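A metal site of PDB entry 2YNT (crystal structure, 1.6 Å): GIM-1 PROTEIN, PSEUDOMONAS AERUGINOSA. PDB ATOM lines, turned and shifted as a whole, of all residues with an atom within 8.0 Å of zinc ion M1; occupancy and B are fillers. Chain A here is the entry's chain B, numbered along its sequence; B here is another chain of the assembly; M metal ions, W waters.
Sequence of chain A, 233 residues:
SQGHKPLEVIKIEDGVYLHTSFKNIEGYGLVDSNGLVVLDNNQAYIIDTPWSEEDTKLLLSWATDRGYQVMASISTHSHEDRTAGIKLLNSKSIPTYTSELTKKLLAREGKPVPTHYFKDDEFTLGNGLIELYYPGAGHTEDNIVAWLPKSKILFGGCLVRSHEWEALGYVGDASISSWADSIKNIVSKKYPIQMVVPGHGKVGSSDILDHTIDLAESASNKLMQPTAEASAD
O of Gly 199 is in hydrogen-bond range of NH2 of Arg 82, 3.4 Å away.
A ring nitrogen (ND1) of His 200 is in hydrogen-bond range of the backbone carbonyl oxygen (O) of Gly 27 of chain B (3.4 Å).
OD2 of Asp 81 lies close to NE of Arg 82, 2.9 Å away.
ND1 of His 200 is in hydrogen-bond range of O of Asp 32 (2.8 Å).
The guanidinium group (NH1) of Arg 82 lies within salt-bridge range of the side-chain carboxylate (OD2) of Asp 48 (2.9 Å).
The guanidinium group (NH1) of Arg 82 sits at hydrogen-bond distance from the backbone carbonyl oxygen (O) of Asn 34, at 2.8 Å.
The guanidinium group of Arg 82 is in hydrogen-bond range of the side-chain hydroxyl of Ser 33, at 2.7 Å.
The side-chain sulfur (SG) of Cys 158 lies close to the guanidinium group (NE) of Arg 82, at 3.5 Å.
Arg 82 touches zinc ion M1 (NE to ZN, 3.8 Å).
The nearest printed residue that does not touch zinc ion M1 is His 77 (4.2 Å).
Zinc ion M1 is bound by water W1 (2.0 Å), a ring nitrogen (NE2) of His 200 (2.0 Å), the side-chain carboxylate (OD2) of Asp 81 (2.0 Å) and the side-chain sulfur (SG) of Cys 158 (2.3 Å).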
ATOM      1  N   ASP A  32      -0.011 -34.681  15.299  1.00  0.00           N
ATOM      2  CA  ASP A  32      -0.186 -34.276  13.904  1.00  0.00           C
ATOM      3  C   ASP A  32      -1.140 -33.097  13.757  1.00  0.00           C
ATOM      4  O   ASP A  32      -1.909 -32.782  14.683  1.00  0.00           O
ATOM      5  CB  ASP A  32      -0.591 -35.441  12.999  1.00  0.00           C
ATOM      6  CG  ASP A  32      -1.917 -36.083  13.387  1.00  0.00           C
ATOM      7  OD1 ASP A  32      -2.724 -35.476  14.117  1.00  0.00           O
ATOM      8  OD2 ASP A  32      -2.164 -37.213  12.916  1.00  0.00           O
ATOM      9  N   SER A  33      -1.059 -32.421  12.618  1.00  0.00           N
ATOM     10  CA  SER A  33      -1.903 -31.261  12.349  1.00  0.00           C
ATOM     11  C   SER A  33      -2.246 -31.275  10.859  1.00  0.00           C
ATOM     12  O   SER A  33      -1.337 -31.306  10.021  1.00  0.00           O
ATOM     13  CB  SER A  33      -1.169 -29.978  12.738  1.00  0.00           C
ATOM     14  OG  SER A  33      -1.973 -28.831  12.521  1.00  0.00           O
ATOM     15  N   ASN A  34      -3.532 -31.217  10.527  1.00  0.00           N
ATOM     16  CA  ASN A  34      -4.004 -31.355   9.144  1.00  0.00           C
ATOM     17  C   ASN A  34      -4.533 -30.069   8.560  1.00  0.00           C
ATOM     18  O   ASN A  34      -5.184 -29.289   9.247  1.00  0.00           O
ATOM     19  CB  ASN A  34      -5.192 -32.318   9.082  1.00  0.00           C
ATOM     20  CG  ASN A  34      -4.865 -33.699   9.588  1.00  0.00           C
ATOM     21  OD1 ASN A  34      -3.819 -34.273   9.257  1.00  0.00           O
ATOM     22  ND2 ASN A  34      -5.758 -34.254  10.391  1.00  0.00           N
ATOM     23  N   ASP A  48      -5.840 -23.890   5.779  1.00  0.00           N
ATOM     24  CA  ASP A  48      -4.887 -23.964   6.879  1.00  0.00           C
ATOM     25  C   ASP A  48      -3.434 -24.235   6.465  1.00  0.00           C
ATOM     26  O   ASP A  48      -3.164 -25.106   5.618  1.00  0.00           O
ATOM     27  CB  ASP A  48      -5.377 -24.906   8.001  1.00  0.00           C
ATOM     28  CG  ASP A  48      -6.553 -24.321   8.744  1.00  0.00           C
ATOM     29  OD1 ASP A  48      -6.575 -23.087   8.927  1.00  0.00           O
ATOM     30  OD2 ASP A  48      -7.453 -25.086   9.139  1.00  0.00           O
ATOM     31  N   TRP A  51       2.148 -26.446  10.239  1.00  0.00           N
ATOM     32  CA  TRP A  51       2.383 -26.017  11.612  1.00  0.00           C
ATOM     33  C   TRP A  51       3.686 -25.220  11.799  1.00  0.00           C
ATOM     34  O   TRP A  51       3.949 -24.656  12.877  1.00  0.00           O
ATOM     35  CB  TRP A  51       2.392 -27.270  12.480  1.00  0.00           C
ATOM     36  CG  TRP A  51       2.082 -27.104  13.947  1.00  0.00           C
ATOM     37  CD1 TRP A  51       1.988 -25.950  14.674  1.00  0.00           C
ATOM     38  CD2 TRP A  51       1.808 -28.176  14.850  1.00  0.00           C
ATOM     39  NE1 TRP A  51       1.681 -26.255  15.998  1.00  0.00           N
ATOM     40  CE2 TRP A  51       1.566 -27.611  16.122  1.00  0.00           C
ATOM     41  CE3 TRP A  51       1.751 -29.572  14.707  1.00  0.00           C
ATOM     42  CZ2 TRP A  51       1.274 -28.406  17.242  1.00  0.00           C
ATOM     43  CZ3 TRP A  51       1.459 -30.352  15.817  1.00  0.00           C
ATOM     44  CH2 TRP A  51       1.225 -29.765  17.061  1.00  0.00           C
ATOM     45  N   THR A  76      -8.388 -21.235   9.600  1.00  0.00           N
ATOM     46  CA  THR A  76      -9.713 -21.457  10.209  1.00  0.00           C
ATOM     47  C   THR A  76      -9.832 -21.060  11.686  1.00  0.00           C
ATOM     48  O   THR A  76     -10.915 -21.132  12.268  1.00  0.00           O
ATOM     49  CB  THR A  76     -10.181 -22.912  10.005  1.00  0.00           C
ATOM     50  OG1 THR A  76      -9.242 -23.812  10.609  1.00  0.00           O
ATOM     51  CG2 THR A  76     -10.301 -23.217   8.513  1.00  0.00           C
ATOM     52  N   HIS A  77      -8.706 -20.665  12.281  1.00  0.00           N
ATOM     53  CA  HIS A  77      -8.680 -19.892  13.528  1.00  0.00           C
ATOM     54  C   HIS A  77      -7.253 -19.436  13.744  1.00  0.00           C
ATOM     55  O   HIS A  77      -6.393 -19.719  12.916  1.00  0.00           O
ATOM     56  CB  HIS A  77      -9.268 -20.637  14.768  1.00  0.00           C
ATOM     57  CG  HIS A  77      -8.531 -21.878  15.188  1.00  0.00           C
ATOM     58  ND1 HIS A  77      -8.719 -23.101  14.579  1.00  0.00           N
ATOM     59  CD2 HIS A  77      -7.678 -22.099  16.217  1.00  0.00           C
ATOM     60  CE1 HIS A  77      -7.986 -24.021  15.188  1.00  0.00           C
ATOM     61  NE2 HIS A  77      -7.341 -23.438  16.184  1.00  0.00           N
ATOM     62  N   HIS A  79      -4.788 -20.035  16.033  1.00  0.00           N
ATOM     63  CA  HIS A  79      -3.717 -20.848  16.599  1.00  0.00           C
ATOM     64  C   HIS A  79      -2.590 -21.111  15.590  1.00  0.00           C
ATOM     65  O   HIS A  79      -2.836 -21.182  14.367  1.00  0.00           O
ATOM     66  CB  HIS A  79      -4.275 -22.170  17.124  1.00  0.00           C
ATOM     67  CG  HIS A  79      -4.997 -22.038  18.429  1.00  0.00           C
ATOM     68  ND1 HIS A  79      -5.855 -23.008  18.882  1.00  0.00           N
ATOM     69  CD2 HIS A  79      -4.968 -21.067  19.371  1.00  0.00           C
ATOM     70  CE1 HIS A  79      -6.340 -22.632  20.060  1.00  0.00           C
ATOM     71  NE2 HIS A  79      -5.807 -21.474  20.382  1.00  0.00           N
ATOM     72  N   GLU A  80      -1.369 -21.262  16.106  1.00  0.00           N
ATOM     73  CA  GLU A  80      -0.186 -21.454  15.254  1.00  0.00           C
ATOM     74  C   GLU A  80      -0.308 -22.650  14.299  1.00  0.00           C
ATOM     75  O   GLU A  80       0.220 -22.599  13.175  1.00  0.00           O
ATOM     76  CB  GLU A  80       1.057 -21.605  16.132  1.00  0.00           C
ATOM     77  CG  GLU A  80       2.374 -21.656  15.374  1.00  0.00           C
ATOM     78  OE1 GLU A  80       3.353 -22.326  17.442  1.00  0.00           O
ATOM     79  OE2 GLU A  80       4.698 -21.591  15.875  1.00  0.00           O
ATOM     80  N   ASP A  81      -0.994 -23.715  14.711  1.00  0.00           N
ATOM     81  CA  ASP A  81      -1.122 -24.871  13.817  1.00  0.00           C
ATOM     82  C   ASP A  81      -2.007 -24.591  12.597  1.00  0.00           C
ATOM     83  O   ASP A  81      -2.013 -25.384  11.672  1.00  0.00           O
ATOM     84  CB  ASP A  81      -1.557 -26.147  14.562  1.00  0.00           C
ATOM     85  CG  ASP A  81      -2.869 -26.003  15.283  1.00  0.00           C
ATOM     86  OD1 ASP A  81      -2.910 -25.300  16.323  1.00  0.00           O
ATOM     87  OD2 ASP A  81      -3.872 -26.627  14.842  1.00  0.00           O
ATOM     88  N   ARG A  82      -2.726 -23.472  12.596  1.00  0.00           N
ATOM     89  CA  ARG A  82      -3.522 -23.075  11.426  1.00  0.00           C
ATOM     90  C   ARG A  82      -2.849 -21.987  10.592  1.00  0.00           C
ATOM     91  O   ARG A  82      -3.230 -21.770   9.427  1.00  0.00           O
ATOM     92  CB  ARG A  82      -4.887 -22.522  11.864  1.00  0.00           C
ATOM     93  CG  ARG A  82      -5.709 -23.381  12.803  1.00  0.00           C
ATOM     94  CD  ARG A  82      -6.211 -24.643  12.150  1.00  0.00           C
ATOM     95  NE  ARG A  82      -5.312 -25.771  12.415  1.00  0.00           N
ATOM     96  CZ  ARG A  82      -5.324 -26.918  11.750  1.00  0.00           C
ATOM     97  NH1 ARG A  82      -6.154 -27.093  10.732  1.00  0.00           N
ATOM     98  NH2 ARG A  82      -4.490 -27.889  12.104  1.00  0.00           N
ATOM     99  N   HIS A 139     -13.964 -24.960  19.924  1.00  0.00           N
ATOM    100  CA  HIS A 139     -12.532 -25.099  20.164  1.00  0.00           C
ATOM    101  C   HIS A 139     -11.910 -23.722  20.459  1.00  0.00           C
ATOM    102  O   HIS A 139     -11.085 -23.574  21.385  1.00  0.00           O
ATOM    103  CB  HIS A 139     -11.892 -25.726  18.930  1.00  0.00           C
ATOM    104  CG  HIS A 139     -10.403 -25.679  18.929  1.00  0.00           C
ATOM    105  ND1 HIS A 139      -9.633 -26.501  19.724  1.00  0.00           N
ATOM    106  CD2 HIS A 139      -9.540 -24.895  18.251  1.00  0.00           C
ATOM    107  CE1 HIS A 139      -8.348 -26.227  19.514  1.00  0.00           C
ATOM    108  NE2 HIS A 139      -8.275 -25.259  18.623  1.00  0.00           N
ATOM    109  N   THR A 140     -12.286 -22.727  19.667  1.00  0.00           N
ATOM    110  CA  THR A 140     -11.978 -21.327  19.959  1.00  0.00           C
ATOM    111  C   THR A 140     -13.194 -20.451  19.664  1.00  0.00           C
ATOM    112  O   THR A 140     -14.214 -20.932  19.145  1.00  0.00           O
ATOM    113  CB  THR A 140     -10.816 -20.804  19.105  1.00  0.00           C
ATOM    114  OG1 THR A 140     -11.112 -21.031  17.723  1.00  0.00           O
ATOM    115  CG2 THR A 140      -9.511 -21.500  19.491  1.00  0.00           C
ATOM    116  N   GLY A 157     -11.806 -28.761  10.787  1.00  0.00           N
ATOM    117  CA  GLY A 157     -10.711 -28.138  11.526  1.00  0.00           C
ATOM    118  C   GLY A 157     -10.727 -28.605  12.966  1.00  0.00           C
ATOM    119  O   GLY A 157     -11.182 -29.717  13.283  1.00  0.00           O
ATOM    120  N   CYS A 158     -10.253 -27.754  13.857  1.00  0.00           N
ATOM    121  CA  CYS A 158      -9.982 -28.188  15.228  1.00  0.00           C
ATOM    122  C   CYS A 158     -11.228 -28.142  16.092  1.00  0.00           C
ATOM    123  O   CYS A 158     -11.218 -28.565  17.254  1.00  0.00           O
ATOM    124  CB  CYS A 158      -8.839 -27.339  15.806  1.00  0.00           C
ATOM    125  SG  CYS A 158      -7.384 -27.374  14.707  1.00  0.00           S
ATOM    126  N   LEU A 159     -12.321 -27.656  15.515  1.00  0.00           N
ATOM    127  CA  LEU A 159     -13.625 -27.672  16.152  1.00  0.00           C
ATOM    128  C   LEU A 159     -14.201 -29.083  16.231  1.00  0.00           C
ATOM    129  O   LEU A 159     -15.050 -29.359  17.075  1.00  0.00           O
ATOM    130  CB  LEU A 159     -14.593 -26.769  15.375  1.00  0.00           C
ATOM    131  CG  LEU A 159     -16.063 -26.698  15.792  1.00  0.00           C
ATOM    132  CD1 LEU A 159     -16.215 -26.145  17.210  1.00  0.00           C
ATOM    133  CD2 LEU A 159     -16.814 -25.834  14.798  1.00  0.00           C
ATOM    134  N   ARG A 161     -13.712 -33.425  16.517  1.00  0.00           N
ATOM    135  CA  ARG A 161     -12.799 -34.383  17.128  1.00  0.00           C
ATOM    136  C   ARG A 161     -12.919 -35.771  16.489  1.00  0.00           C
ATOM    137  O   ARG A 161     -13.998 -36.339  16.445  1.00  0.00           O
ATOM    138  CB  ARG A 161     -13.041 -34.483  18.643  1.00  0.00           C
ATOM    139  CG  ARG A 161     -12.867 -33.165  19.384  1.00  0.00           C
ATOM    140  CD  ARG A 161     -11.394 -32.714  19.363  1.00  0.00           C
ATOM    141  NE  ARG A 161     -10.570 -33.563  20.232  1.00  0.00           N
ATOM    142  CZ  ARG A 161      -9.238 -33.540  20.249  1.00  0.00           C
ATOM    143  NH1 ARG A 161      -8.571 -32.730  19.437  1.00  0.00           N
ATOM    144  NH2 ARG A 161      -8.569 -34.341  21.067  1.00  0.00           N
ATOM    145  N   TYR A 170      -6.954 -29.562  23.283  1.00  0.00           N
ATOM    146  CA  TYR A 170      -6.535 -28.319  23.930  1.00  0.00           C
ATOM    147  C   TYR A 170      -7.713 -27.359  24.102  1.00  0.00           C
ATOM    148  O   TYR A 170      -8.324 -26.941  23.116  1.00  0.00           O
ATOM    149  CB  TYR A 170      -5.417 -27.631  23.148  1.00  0.00           C
ATOM    150  CG  TYR A 170      -5.001 -26.316  23.776  1.00  0.00           C
ATOM    151  CD1 TYR A 170      -4.199 -26.302  24.918  1.00  0.00           C
ATOM    152  CD2 TYR A 170      -5.409 -25.088  23.239  1.00  0.00           C
ATOM    153  CE1 TYR A 170      -3.822 -25.110  25.510  1.00  0.00           C
ATOM    154  CE2 TYR A 170      -5.026 -23.888  23.822  1.00  0.00           C
ATOM    155  CZ  TYR A 170      -4.243 -23.910  24.961  1.00  0.00           C
ATOM    156  OH  TYR A 170      -3.851 -22.731  25.544  1.00  0.00           O
ATOM    157  N   PRO A 198     -10.617 -33.575  10.338  1.00  0.00           N
ATOM    158  CA  PRO A 198     -10.354 -32.837  11.571  1.00  0.00           C
ATOM    159  C   PRO A 198      -8.997 -32.144  11.498  1.00  0.00           C
ATOM    160  O   PRO A 198      -8.168 -32.521  10.665  1.00  0.00           O
ATOM    161  CB  PRO A 198     -10.305 -33.929  12.638  1.00  0.00           C
ATOM    162  CG  PRO A 198      -9.725 -35.123  11.884  1.00  0.00           C
ATOM    163  CD  PRO A 198     -10.208 -34.991  10.439  1.00  0.00           C
ATOM    164  N   GLY A 199      -8.792 -31.160  12.363  1.00  0.00           N
ATOM    165  CA  GLY A 199      -7.525 -30.454  12.435  1.00  0.00           C
ATOM    166  C   GLY A 199      -6.436 -31.337  13.001  1.00  0.00           C
ATOM    167  O   GLY A 199      -5.259 -31.145  12.690  1.00  0.00           O
ATOM    168  N   HIS A 200      -6.811 -32.286  13.840  1.00  0.00           N
ATOM    169  CA  HIS A 200      -5.851 -33.206  14.445  1.00  0.00           C
ATOM    170  C   HIS A 200      -6.436 -34.602  14.444  1.00  0.00           C
ATOM    171  O   HIS A 200      -7.597 -34.802  14.826  1.00  0.00           O
ATOM    172  CB  HIS A 200      -5.521 -32.759  15.876  1.00  0.00           C
ATOM    173  CG  HIS A 200      -5.057 -31.345  15.969  1.00  0.00           C
ATOM    174  ND1 HIS A 200      -3.771 -30.955  15.652  1.00  0.00           N
ATOM    175  CD2 HIS A 200      -5.712 -30.209  16.334  1.00  0.00           C
ATOM    176  CE1 HIS A 200      -3.660 -29.648  15.807  1.00  0.00           C
ATOM    177  NE2 HIS A 200      -4.821 -29.168  16.227  1.00  0.00           N
ATOM    178  N   GLU B  26      -0.748 -26.747  23.180  1.00  0.00           N
ATOM    179  CA  GLU B  26      -1.579 -26.388  22.036  1.00  0.00           C
ATOM    180  C   GLU B  26      -1.323 -27.409  20.923  1.00  0.00           C
ATOM    181  O   GLU B  26      -0.188 -27.860  20.722  1.00  0.00           O
ATOM    182  CB  GLU B  26      -1.243 -24.967  21.549  1.00  0.00           C
ATOM    183  CG  GLU B  26      -2.449 -24.131  21.163  1.00  0.00           C
ATOM    184  CD  GLU B  26      -2.059 -22.722  20.720  1.00  0.00           C
ATOM    185  OE1 GLU B  26      -1.578 -22.574  19.575  1.00  0.00           O
ATOM    186  OE2 GLU B  26      -2.223 -21.781  21.526  1.00  0.00           O
ATOM    187  N   GLY B  27      -2.371 -27.796  20.225  1.00  0.00           N
ATOM    188  CA  GLY B  27      -2.235 -28.813  19.203  1.00  0.00           C
ATOM    189  C   GLY B  27      -2.593 -30.179  19.751  1.00  0.00           C
ATOM    190  O   GLY B  27      -2.946 -31.068  18.978  1.00  0.00           O
ATOM    191  N   TYR B  28      -2.517 -30.354  21.066  1.00  0.00           N
ATOM    192  CA  TYR B  28      -2.878 -31.645  21.685  1.00  0.00           C
ATOM    193  C   TYR B  28      -3.779 -31.537  22.927  1.00  0.00           C
ATOM    194  O   TYR B  28      -4.825 -32.197  22.993  1.00  0.00           O
ATOM    195  CB  TYR B  28      -1.641 -32.478  22.033  1.00  0.00           C
ATOM    196  CG  TYR B  28      -2.030 -33.751  22.741  1.00  0.00           C
ATOM    197  CD1 TYR B  28      -2.569 -34.816  22.041  1.00  0.00           C
ATOM    198  CD2 TYR B  28      -1.906 -33.868  24.121  1.00  0.00           C
ATOM    199  CE1 TYR B  28      -2.969 -35.968  22.682  1.00  0.00           C
ATOM    200  CE2 TYR B  28      -2.291 -35.019  24.773  1.00  0.00           C
ATOM    201  CZ  TYR B  28      -2.823 -36.062  24.044  1.00  0.00           C
ATOM    202  OH  TYR B  28      -3.208 -37.213  24.686  1.00  0.00           O
HETATM  203 ZN    ZN M   1      -5.485 -27.267  15.921  1.00  0.00          ZN
HETATM  204 ZN    ZN M   2      -6.593 -24.500  17.763  1.00  0.00          ZN
HETATM  205  O   HOH W   1      -5.364 -25.906  17.432  1.00  0.00           O
